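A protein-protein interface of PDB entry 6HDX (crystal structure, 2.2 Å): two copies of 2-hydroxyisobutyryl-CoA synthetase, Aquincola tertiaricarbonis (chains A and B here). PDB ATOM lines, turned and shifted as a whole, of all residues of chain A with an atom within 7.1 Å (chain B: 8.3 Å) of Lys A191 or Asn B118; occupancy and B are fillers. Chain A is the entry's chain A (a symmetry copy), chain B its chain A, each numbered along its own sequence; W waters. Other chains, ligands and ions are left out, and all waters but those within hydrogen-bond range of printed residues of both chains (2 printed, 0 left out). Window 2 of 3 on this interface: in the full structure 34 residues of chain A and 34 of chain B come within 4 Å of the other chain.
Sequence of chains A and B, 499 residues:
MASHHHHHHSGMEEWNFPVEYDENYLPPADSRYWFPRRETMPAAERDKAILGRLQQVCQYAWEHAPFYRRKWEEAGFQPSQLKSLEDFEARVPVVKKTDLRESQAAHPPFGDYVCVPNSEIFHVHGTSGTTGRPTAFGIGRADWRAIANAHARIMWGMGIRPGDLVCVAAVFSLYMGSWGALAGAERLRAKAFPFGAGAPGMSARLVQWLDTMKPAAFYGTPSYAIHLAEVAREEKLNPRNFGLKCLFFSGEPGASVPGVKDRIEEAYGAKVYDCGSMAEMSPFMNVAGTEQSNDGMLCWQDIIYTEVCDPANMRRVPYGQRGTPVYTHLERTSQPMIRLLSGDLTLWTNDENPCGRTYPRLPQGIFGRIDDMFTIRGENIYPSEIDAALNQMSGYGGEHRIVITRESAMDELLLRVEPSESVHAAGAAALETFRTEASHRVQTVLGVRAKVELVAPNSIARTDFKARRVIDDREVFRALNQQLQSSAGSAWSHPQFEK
NZ of Lys A191 lies close to ND2 of Asn B118, at 3.1 Å.
The backbone carbonyl oxygen of Ala A192 is in hydrogen-bond range of the backbone NH of Val B124, 2.8 Å away.
NE2 of His B123 sits at hydrogen-bond distance from OE2 of Glu A186.
The backbone carbonyl oxygen of Phe B122 is in hydrogen-bond range of the backbone NH of Ala A192.
O of Ile B139 lies within hydrogen-bond range of N of Phe B122 (2.8 Å).
The backbone NH (N) of Lys A191 sits at hydrogen-bond distance from the backbone carbonyl oxygen (O) of Asp A164 (2.7 Å).
The backbone NH (N) of Ala A190 sits at hydrogen-bond distance from the backbone carbonyl oxygen (O) of Ala A185, 3.0 Å away.
The side-chain amino group of Lys A191 is in hydrogen-bond range of the backbone carbonyl oxygen of Gly A163 (2.8 Å).
O of His B123 is in hydrogen-bond range of N of Ile B139.
The backbone carbonyl oxygen (O) of Lys A191 lies within hydrogen-bond range of the backbone NH (N) of Val A166.
Among the printed residues, pairs that only touch across the chains: Leu A165 with Val B124, Glu A186 with Phe B122, Ala A190 with Ile B121, Ala A190 with Phe B122, Lys A191 with Ile B121, Lys A191 with Phe B122, Ala A192 with His B123, Phe A193 with Val B124 and Pro A194 with Val B124.
Lys A191 touches just these residues of chain B: Asn B118, Ile B121 and Phe B122.
Of the printed residues of chain B, Ala A192 touches Phe B122, His B123 and Val B124.
Of the printed residues of chain B, Pro A194 touches Val B124 (3.5 Å).
Asn B118 touches just one residue of chain A: Lys A191.
Printed residues of chain A within 4 Å of Ile B121: Ala A190 and Lys A191.
Of the printed residues of chain A, Phe B122 touches Glu A186 (3.6 Å), Ala A190 (3.8 Å), Lys A191 (3.9 Å) and Ala A192 (3.0 Å).
Printed residues of chain A within 4 Å of His B123: Glu A186 and Ala A192.
The nearest residue of chain A that does not touch Asn B118 is Gly A163 (5.2 Å).
The nearest printed residue of chain A that does not touch His B123 is Pro A194 (4.04 Å).
Of the 17 printed residues of chain B, 5 touch a printed residue of chain A.
Printed residues of chain A that touch a printed residue of chain B: Leu A165, Glu A186, Ala A190, Lys A191, Ala A192, Phe A193 and Pro A194.
Hydrophobic or aromatic side chains of chain A within 4 Å of the printed part of chain B: Leu A165, Ala A192, Phe A193 and Pro A194.
Among the printed residues, 13 pairs touch across the chains.
Among the printed residues, no Asp or Glu carboxylate lies within 4 Å of a Lys or Arg side-chain nitrogen of the other chain.
No position is printed for both chains.
Of the 13 pairs that touch across the chains among the printed residues, none has its exchanged pair printed and touching as well.
Water W2 lies within hydrogen-bond range of O of Val B124 (2.8 Å) and O of Pro A194 (3.3 Å).
Water W1 lies within hydrogen-bond range of the backbone carbonyl oxygen (O) of Ile B121 (3.2 Å) and the backbone carbonyl oxygen (O) of Ala A190 (3.3 Å).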
ATOM      1  N   ARG A 161      -3.147  -3.473  28.571  1.00  0.00           N
ATOM      2  CA  ARG A 161      -1.781  -3.984  28.509  1.00  0.00           C
ATOM      3  C   ARG A 161      -1.096  -3.822  27.159  1.00  0.00           C
ATOM      4  O   ARG A 161      -1.797  -3.703  26.153  1.00  0.00           O
ATOM      5  CB  ARG A 161      -1.800  -5.495  28.900  1.00  0.00           C
ATOM      6  CG  ARG A 161      -2.252  -5.807  30.348  1.00  0.00           C
ATOM      7  CD  ARG A 161      -1.162  -5.498  31.370  1.00  0.00           C
ATOM      8  NE  ARG A 161      -1.571  -5.754  32.767  1.00  0.00           N
ATOM      9  CZ  ARG A 161      -2.146  -4.853  33.550  1.00  0.00           C
ATOM     10  NH1 ARG A 161      -2.453  -3.647  33.076  1.00  0.00           N
ATOM     11  NH2 ARG A 161      -2.455  -5.158  34.803  1.00  0.00           N
ATOM     12  N   PRO A 162       0.272  -3.909  27.103  1.00  0.00           N
ATOM     13  CA  PRO A 162       0.963  -3.888  25.798  1.00  0.00           C
ATOM     14  C   PRO A 162       0.413  -4.961  24.853  1.00  0.00           C
ATOM     15  O   PRO A 162       0.088  -6.076  25.294  1.00  0.00           O
ATOM     16  CB  PRO A 162       2.427  -4.199  26.153  1.00  0.00           C
ATOM     17  CG  PRO A 162       2.576  -3.788  27.573  1.00  0.00           C
ATOM     18  CD  PRO A 162       1.237  -4.053  28.217  1.00  0.00           C
ATOM     19  N   GLY A 163       0.250  -4.592  23.578  1.00  0.00           N
ATOM     20  CA  GLY A 163      -0.282  -5.495  22.564  1.00  0.00           C
ATOM     21  C   GLY A 163      -1.793  -5.497  22.437  1.00  0.00           C
ATOM     22  O   GLY A 163      -2.319  -6.049  21.470  1.00  0.00           O
ATOM     23  N   ASP A 164      -2.511  -4.938  23.429  1.00  0.00           N
ATOM     24  CA  ASP A 164      -3.974  -4.815  23.357  1.00  0.00           C
ATOM     25  C   ASP A 164      -4.354  -3.783  22.280  1.00  0.00           C
ATOM     26  O   ASP A 164      -3.751  -2.714  22.191  1.00  0.00           O
ATOM     27  CB  ASP A 164      -4.538  -4.304  24.676  1.00  0.00           C
ATOM     28  CG  ASP A 164      -4.685  -5.325  25.786  1.00  0.00           C
ATOM     29  OD1 ASP A 164      -4.561  -6.550  25.502  1.00  0.00           O
ATOM     30  OD2 ASP A 164      -5.005  -4.914  26.915  1.00  0.00           O
ATOM     31  N   LEU A 165      -5.362  -4.108  21.482  1.00  0.00           N
ATOM     32  CA  LEU A 165      -5.910  -3.218  20.487  1.00  0.00           C
ATOM     33  C   LEU A 165      -6.825  -2.207  21.211  1.00  0.00           C
ATOM     34  O   LEU A 165      -7.810  -2.605  21.849  1.00  0.00           O
ATOM     35  CB  LEU A 165      -6.687  -4.019  19.437  1.00  0.00           C
ATOM     36  CG  LEU A 165      -7.206  -3.182  18.247  1.00  0.00           C
ATOM     37  CD1 LEU A 165      -6.078  -2.770  17.353  1.00  0.00           C
ATOM     38  CD2 LEU A 165      -8.209  -3.962  17.440  1.00  0.00           C
ATOM     39  N   VAL A 166      -6.456  -0.908  21.160  1.00  0.00           N
ATOM     40  CA  VAL A 166      -7.210   0.169  21.819  1.00  0.00           C
ATOM     41  C   VAL A 166      -7.852   1.064  20.771  1.00  0.00           C
ATOM     42  O   VAL A 166      -7.138   1.775  20.060  1.00  0.00           O
ATOM     43  CB  VAL A 166      -6.329   0.993  22.809  1.00  0.00           C
ATOM     44  CG1 VAL A 166      -7.118   2.150  23.432  1.00  0.00           C
ATOM     45  CG2 VAL A 166      -5.732   0.097  23.893  1.00  0.00           C
ATOM     46  N   CYS A 167      -9.185   1.015  20.667  1.00  0.00           N
ATOM     47  CA  CYS A 167      -9.913   1.870  19.740  1.00  0.00           C
ATOM     48  C   CYS A 167     -10.143   3.250  20.362  1.00  0.00           C
ATOM     49  O   CYS A 167     -10.834   3.343  21.366  1.00  0.00           O
ATOM     50  CB  CYS A 167     -11.234   1.230  19.301  1.00  0.00           C
ATOM     51  SG  CYS A 167     -12.170   2.233  18.111  1.00  0.00           S
ATOM     52  N   ALA A 185      -2.039   5.110  24.762  1.00  0.00           N
ATOM     53  CA  ALA A 185      -2.045   3.824  24.045  1.00  0.00           C
ATOM     54  C   ALA A 185      -0.694   3.556  23.392  1.00  0.00           C
ATOM     55  O   ALA A 185      -0.196   2.433  23.464  1.00  0.00           O
ATOM     56  CB  ALA A 185      -3.155   3.802  22.995  1.00  0.00           C
ATOM     57  N   GLU A 186      -0.094   4.598  22.762  1.00  0.00           N
ATOM     58  CA  GLU A 186       1.222   4.553  22.116  1.00  0.00           C
ATOM     59  C   GLU A 186       2.321   4.193  23.120  1.00  0.00           C
ATOM     60  O   GLU A 186       3.099   3.264  22.866  1.00  0.00           O
ATOM     61  CB  GLU A 186       1.543   5.914  21.474  1.00  0.00           C
ATOM     62  CG  GLU A 186       0.779   6.204  20.177  1.00  0.00           C
ATOM     63  CD  GLU A 186       0.945   7.599  19.595  1.00  0.00           C
ATOM     64  OE1 GLU A 186       1.488   8.486  20.286  1.00  0.00           O
ATOM     65  OE2 GLU A 186       0.497   7.820  18.452  1.00  0.00           O
ATOM     66  N   LEU A 188       1.972   2.854  26.205  1.00  0.00           N
ATOM     67  CA  LEU A 188       1.663   1.552  26.811  1.00  0.00           C
ATOM     68  C   LEU A 188       2.093   0.373  25.899  1.00  0.00           C
ATOM     69  O   LEU A 188       2.039  -0.791  26.313  1.00  0.00           O
ATOM     70  CB  LEU A 188       0.133   1.506  27.078  1.00  0.00           C
ATOM     71  CG  LEU A 188      -0.454   0.257  27.787  1.00  0.00           C
ATOM     72  CD1 LEU A 188       0.280  -0.035  29.104  1.00  0.00           C
ATOM     73  CD2 LEU A 188      -1.957   0.447  28.006  1.00  0.00           C
ATOM     74  N   ARG A 189       2.513   0.686  24.653  1.00  0.00           N
ATOM     75  CA  ARG A 189       2.879  -0.276  23.602  1.00  0.00           C
ATOM     76  C   ARG A 189       1.652  -1.126  23.230  1.00  0.00           C
ATOM     77  O   ARG A 189       1.758  -2.306  22.917  1.00  0.00           O
ATOM     78  CB  ARG A 189       4.137  -1.124  23.922  1.00  0.00           C
ATOM     79  CG  ARG A 189       5.293  -0.369  24.577  1.00  0.00           C
ATOM     80  CD  ARG A 189       6.228   0.253  23.582  1.00  0.00           C
ATOM     81  NE  ARG A 189       6.361   1.698  23.776  1.00  0.00           N
ATOM     82  CZ  ARG A 189       7.349   2.280  24.448  1.00  0.00           C
ATOM     83  NH1 ARG A 189       7.405   3.602  24.541  1.00  0.00           N
ATOM     84  NH2 ARG A 189       8.291   1.545  25.026  1.00  0.00           N
ATOM     85  N   ALA A 190       0.467  -0.503  23.283  1.00  0.00           N
ATOM     86  CA  ALA A 190      -0.777  -1.143  22.864  1.00  0.00           C
ATOM     87  C   ALA A 190      -0.822  -0.984  21.337  1.00  0.00           C
ATOM     88  O   ALA A 190       0.003  -0.263  20.779  1.00  0.00           O
ATOM     89  CB  ALA A 190      -1.976  -0.428  23.508  1.00  0.00           C
ATOM     90  N   LYS A 191      -1.749  -1.652  20.659  1.00  0.00           N
ATOM     91  CA  LYS A 191      -1.932  -1.423  19.225  1.00  0.00           C
ATOM     92  C   LYS A 191      -2.905  -0.226  19.130  1.00  0.00           C
ATOM     93  O   LYS A 191      -4.109  -0.412  19.294  1.00  0.00           O
ATOM     94  CB  LYS A 191      -2.545  -2.649  18.539  1.00  0.00           C
ATOM     95  CG  LYS A 191      -1.632  -3.836  18.414  1.00  0.00           C
ATOM     96  CD  LYS A 191      -2.471  -5.050  18.078  1.00  0.00           C
ATOM     97  CE  LYS A 191      -1.632  -6.278  17.856  1.00  0.00           C
ATOM     98  NZ  LYS A 191      -1.060  -6.818  19.127  1.00  0.00           N
ATOM     99  N   ALA A 192      -2.384   1.008  18.995  1.00  0.00           N
ATOM    100  CA  ALA A 192      -3.267   2.198  18.960  1.00  0.00           C
ATOM    101  C   ALA A 192      -4.096   2.216  17.694  1.00  0.00           C
ATOM    102  O   ALA A 192      -3.540   2.199  16.601  1.00  0.00           O
ATOM    103  CB  ALA A 192      -2.454   3.486  19.068  1.00  0.00           C
ATOM    104  N   PHE A 193      -5.432   2.225  17.838  1.00  0.00           N
ATOM    105  CA  PHE A 193      -6.351   2.262  16.698  1.00  0.00           C
ATOM    106  C   PHE A 193      -7.129   3.615  16.722  1.00  0.00           C
ATOM    107  O   PHE A 193      -8.258   3.673  17.223  1.00  0.00           O
ATOM    108  CB  PHE A 193      -7.262   1.011  16.726  1.00  0.00           C
ATOM    109  CG  PHE A 193      -8.355   0.910  15.695  1.00  0.00           C
ATOM    110  CD1 PHE A 193      -8.183   1.439  14.412  1.00  0.00           C
ATOM    111  CD2 PHE A 193      -9.554   0.263  15.991  1.00  0.00           C
ATOM    112  CE1 PHE A 193      -9.196   1.329  13.450  1.00  0.00           C
ATOM    113  CE2 PHE A 193     -10.567   0.147  15.027  1.00  0.00           C
ATOM    114  CZ  PHE A 193     -10.384   0.684  13.765  1.00  0.00           C
ATOM    115  N   PRO A 194      -6.532   4.721  16.195  1.00  0.00           N
ATOM    116  CA  PRO A 194      -7.232   6.017  16.242  1.00  0.00           C
ATOM    117  C   PRO A 194      -8.251   6.216  15.119  1.00  0.00           C
ATOM    118  O   PRO A 194      -8.009   6.925  14.143  1.00  0.00           O
ATOM    119  CB  PRO A 194      -6.088   7.028  16.228  1.00  0.00           C
ATOM    120  CG  PRO A 194      -4.958   6.335  15.487  1.00  0.00           C
ATOM    121  CD  PRO A 194      -5.198   4.852  15.556  1.00  0.00           C
ATOM    122  N   PRO B 108      -6.378 -12.996   8.750  1.00  0.00           N
ATOM    123  CA  PRO B 108      -6.763 -11.760   9.428  1.00  0.00           C
ATOM    124  C   PRO B 108      -5.959 -11.441  10.687  1.00  0.00           C
ATOM    125  O   PRO B 108      -5.492 -12.351  11.362  1.00  0.00           O
ATOM    126  CB  PRO B 108      -8.249 -11.992   9.741  1.00  0.00           C
ATOM    127  CG  PRO B 108      -8.385 -13.442   9.898  1.00  0.00           C
ATOM    128  CD  PRO B 108      -7.364 -14.078   9.001  1.00  0.00           C
ATOM    129  N   PRO B 109      -5.813 -10.157  11.053  1.00  0.00           N
ATOM    130  CA  PRO B 109      -6.341  -8.959  10.381  1.00  0.00           C
ATOM    131  C   PRO B 109      -5.448  -8.253   9.354  1.00  0.00           C
ATOM    132  O   PRO B 109      -5.978  -7.477   8.548  1.00  0.00           O
ATOM    133  CB  PRO B 109      -6.659  -8.035  11.560  1.00  0.00           C
ATOM    134  CG  PRO B 109      -5.677  -8.435  12.660  1.00  0.00           C
ATOM    135  CD  PRO B 109      -5.149  -9.815  12.327  1.00  0.00           C
ATOM    136  N   PHE B 110      -4.122  -8.486   9.370  1.00  0.00           N
ATOM    137  CA  PHE B 110      -3.154  -7.763   8.542  1.00  0.00           C
ATOM    138  C   PHE B 110      -2.593  -8.487   7.300  1.00  0.00           C
ATOM    139  O   PHE B 110      -1.841  -7.871   6.530  1.00  0.00           O
ATOM    140  CB  PHE B 110      -1.997  -7.296   9.438  1.00  0.00           C
ATOM    141  CG  PHE B 110      -2.516  -6.451  10.578  1.00  0.00           C
ATOM    142  CD1 PHE B 110      -3.284  -5.315  10.331  1.00  0.00           C
ATOM    143  CD2 PHE B 110      -2.297  -6.828  11.902  1.00  0.00           C
ATOM    144  CE1 PHE B 110      -3.830  -4.574  11.388  1.00  0.00           C
ATOM    145  CE2 PHE B 110      -2.814  -6.066  12.954  1.00  0.00           C
ATOM    146  CZ  PHE B 110      -3.562  -4.929  12.688  1.00  0.00           C
ATOM    147  N   VAL B 114       2.368  -9.094   6.748  1.00  0.00           N
ATOM    148  CA  VAL B 114       2.614  -8.252   7.930  1.00  0.00           C
ATOM    149  C   VAL B 114       4.119  -8.252   8.345  1.00  0.00           C
ATOM    150  O   VAL B 114       4.641  -7.184   8.669  1.00  0.00           O
ATOM    151  CB  VAL B 114       1.655  -8.555   9.114  1.00  0.00           C
ATOM    152  CG1 VAL B 114       1.878  -9.963   9.706  1.00  0.00           C
ATOM    153  CG2 VAL B 114       1.748  -7.479  10.191  1.00  0.00           C
ATOM    154  N   CYS B 115       4.798  -9.433   8.317  1.00  0.00           N
ATOM    155  CA  CYS B 115       6.231  -9.650   8.579  1.00  0.00           C
ATOM    156  C   CYS B 115       6.626  -9.509  10.037  1.00  0.00           C
ATOM    157  O   CYS B 115       7.313 -10.372  10.550  1.00  0.00           O
ATOM    158  CB  CYS B 115       7.105  -8.760   7.694  1.00  0.00           C
ATOM    159  SG  CYS B 115       7.001  -9.120   5.927  1.00  0.00           S
ATOM    160  N   VAL B 116       6.289  -8.372  10.671  1.00  0.00           N
ATOM    161  CA  VAL B 116       6.661  -8.121  12.069  1.00  0.00           C
ATOM    162  C   VAL B 116       5.803  -8.975  13.009  1.00  0.00           C
ATOM    163  O   VAL B 116       4.664  -9.303  12.641  1.00  0.00           O
ATOM    164  CB  VAL B 116       6.564  -6.603  12.445  1.00  0.00           C
ATOM    165  CG1 VAL B 116       7.563  -5.758  11.664  1.00  0.00           C
ATOM    166  CG2 VAL B 116       5.142  -6.055  12.333  1.00  0.00           C
ATOM    167  N   PRO B 117       6.270  -9.295  14.250  1.00  0.00           N
ATOM    168  CA  PRO B 117       5.374 -10.000  15.173  1.00  0.00           C
ATOM    169  C   PRO B 117       4.248  -9.040  15.539  1.00  0.00           C
ATOM    170  O   PRO B 117       4.427  -7.823  15.475  1.00  0.00           O
ATOM    171  CB  PRO B 117       6.255 -10.316  16.389  1.00  0.00           C
ATOM    172  CG  PRO B 117       7.656  -9.989  15.983  1.00  0.00           C
ATOM    173  CD  PRO B 117       7.574  -8.990  14.884  1.00  0.00           C
ATOM    174  N   ASN B 118       3.088  -9.597  15.894  1.00  0.00           N
ATOM    175  CA  ASN B 118       1.882  -8.900  16.342  1.00  0.00           C
ATOM    176  C   ASN B 118       2.208  -7.861  17.433  1.00  0.00           C
ATOM    177  O   ASN B 118       1.682  -6.759  17.400  1.00  0.00           O
ATOM    178  CB  ASN B 118       0.901  -9.937  16.892  1.00  0.00           C
ATOM    179  CG  ASN B 118      -0.541  -9.518  16.888  1.00  0.00           C
ATOM    180  OD1 ASN B 118      -1.082  -9.061  15.872  1.00  0.00           O
ATOM    181  ND2 ASN B 118      -1.212  -9.737  18.016  1.00  0.00           N
ATOM    182  N   SER B 119       3.116  -8.211  18.363  1.00  0.00           N
ATOM    183  CA  SER B 119       3.600  -7.379  19.464  1.00  0.00           C
ATOM    184  C   SER B 119       4.315  -6.092  19.020  1.00  0.00           C
ATOM    185  O   SER B 119       4.484  -5.193  19.839  1.00  0.00           O
ATOM    186  CB  SER B 119       4.517  -8.198  20.375  1.00  0.00           C
ATOM    187  OG  SER B 119       5.737  -8.527  19.731  1.00  0.00           O
ATOM    188  N   GLU B 120       4.757  -5.998  17.748  1.00  0.00           N
ATOM    189  CA  GLU B 120       5.478  -4.819  17.254  1.00  0.00           C
ATOM    190  C   GLU B 120       4.517  -3.736  16.687  1.00  0.00           C
ATOM    191  O   GLU B 120       4.930  -2.575  16.560  1.00  0.00           O
ATOM    192  CB  GLU B 120       6.592  -5.248  16.262  1.00  0.00           C
ATOM    193  CG  GLU B 120       7.047  -4.248  15.194  1.00  0.00           C
ATOM    194  CD  GLU B 120       8.100  -3.187  15.494  1.00  0.00           C
ATOM    195  OE1 GLU B 120       8.522  -3.045  16.666  1.00  0.00           O
ATOM    196  OE2 GLU B 120       8.500  -2.487  14.534  1.00  0.00           O
ATOM    197  N   ILE B 121       3.243  -4.104  16.399  1.00  0.00           N
ATOM    198  CA  ILE B 121       2.250  -3.182  15.824  1.00  0.00           C
ATOM    199  C   ILE B 121       1.969  -2.007  16.787  1.00  0.00           C
ATOM    200  O   ILE B 121       1.659  -2.200  17.978  1.00  0.00           O
ATOM    201  CB  ILE B 121       0.969  -3.896  15.305  1.00  0.00           C
ATOM    202  CG1 ILE B 121       1.346  -4.809  14.096  1.00  0.00           C
ATOM    203  CG2 ILE B 121      -0.116  -2.864  14.860  1.00  0.00           C
ATOM    204  CD1 ILE B 121       0.601  -6.102  14.080  1.00  0.00           C
ATOM    205  N   PHE B 122       2.165  -0.794  16.248  1.00  0.00           N
ATOM    206  CA  PHE B 122       2.044   0.471  16.951  1.00  0.00           C
ATOM    207  C   PHE B 122       0.722   1.209  16.621  1.00  0.00           C
ATOM    208  O   PHE B 122       0.072   1.734  17.520  1.00  0.00           O
ATOM    209  CB  PHE B 122       3.262   1.328  16.570  1.00  0.00           C
ATOM    210  CG  PHE B 122       3.367   2.722  17.150  1.00  0.00           C
ATOM    211  CD1 PHE B 122       3.646   2.915  18.498  1.00  0.00           C
ATOM    212  CD2 PHE B 122       3.266   3.837  16.333  1.00  0.00           C
ATOM    213  CE1 PHE B 122       3.784   4.204  19.023  1.00  0.00           C
ATOM    214  CE2 PHE B 122       3.385   5.127  16.864  1.00  0.00           C
ATOM    215  CZ  PHE B 122       3.692   5.298  18.196  1.00  0.00           C
ATOM    216  N   HIS B 123       0.359   1.281  15.337  1.00  0.00           N
ATOM    217  CA  HIS B 123      -0.860   1.958  14.895  1.00  0.00           C
ATOM    218  C   HIS B 123      -1.637   1.103  13.937  1.00  0.00           C
ATOM    219  O   HIS B 123      -1.051   0.401  13.100  1.00  0.00           O
ATOM    220  CB  HIS B 123      -0.528   3.264  14.173  1.00  0.00           C
ATOM    221  CG  HIS B 123      -0.577   4.500  15.002  1.00  0.00           C
ATOM    222  ND1 HIS B 123      -1.096   5.672  14.494  1.00  0.00           N
ATOM    223  CD2 HIS B 123      -0.038   4.755  16.208  1.00  0.00           C
ATOM    224  CE1 HIS B 123      -0.880   6.593  15.412  1.00  0.00           C
ATOM    225  NE2 HIS B 123      -0.251   6.084  16.463  1.00  0.00           N
ATOM    226  N   VAL B 124      -2.975   1.199  14.051  1.00  0.00           N
ATOM    227  CA  VAL B 124      -3.929   0.548  13.159  1.00  0.00           C
ATOM    228  C   VAL B 124      -4.680   1.635  12.375  1.00  0.00           C
ATOM    229  O   VAL B 124      -5.244   2.556  12.963  1.00  0.00           O
ATOM    230  CB  VAL B 124      -4.884  -0.472  13.850  1.00  0.00           C
ATOM    231  CG1 VAL B 124      -5.822  -1.123  12.830  1.00  0.00           C
ATOM    232  CG2 VAL B 124      -4.091  -1.547  14.599  1.00  0.00           C
ATOM    233  N   GLY B 138      -1.397  -2.384   9.674  1.00  0.00           N
ATOM    234  CA  GLY B 138      -0.782  -2.730  10.943  1.00  0.00           C
ATOM    235  C   GLY B 138       0.636  -2.242  10.821  1.00  0.00           C
ATOM    236  O   GLY B 138       1.474  -2.921  10.235  1.00  0.00           O
ATOM    237  N   ILE B 139       0.887  -1.022  11.286  1.00  0.00           N
ATOM    238  CA  ILE B 139       2.197  -0.377  11.163  1.00  0.00           C
ATOM    239  C   ILE B 139       3.008  -0.493  12.449  1.00  0.00           C
ATOM    240  O   ILE B 139       2.524  -0.104  13.516  1.00  0.00           O
ATOM    241  CB  ILE B 139       2.037   1.085  10.680  1.00  0.00           C
ATOM    242  CG1 ILE B 139       1.013   1.146   9.523  1.00  0.00           C
ATOM    243  CG2 ILE B 139       3.405   1.696  10.296  1.00  0.00           C
ATOM    244  CD1 ILE B 139       0.405   2.442   9.263  1.00  0.00           C
ATOM    245  N   GLY B 140       4.226  -1.025  12.329  1.00  0.00           N
ATOM    246  CA  GLY B 140       5.140  -1.191  13.447  1.00  0.00           C
ATOM    247  C   GLY B 140       5.699   0.131  13.930  1.00  0.00           C
ATOM    248  O   GLY B 140       5.662   1.133  13.210  1.00  0.00           O
HETATM  249  O   HOH W   1       3.267  -0.586  20.175  1.00  0.00           O
HETATM  250  O   HOH W   2      -7.386   4.291  12.315  1.00  0.00           O
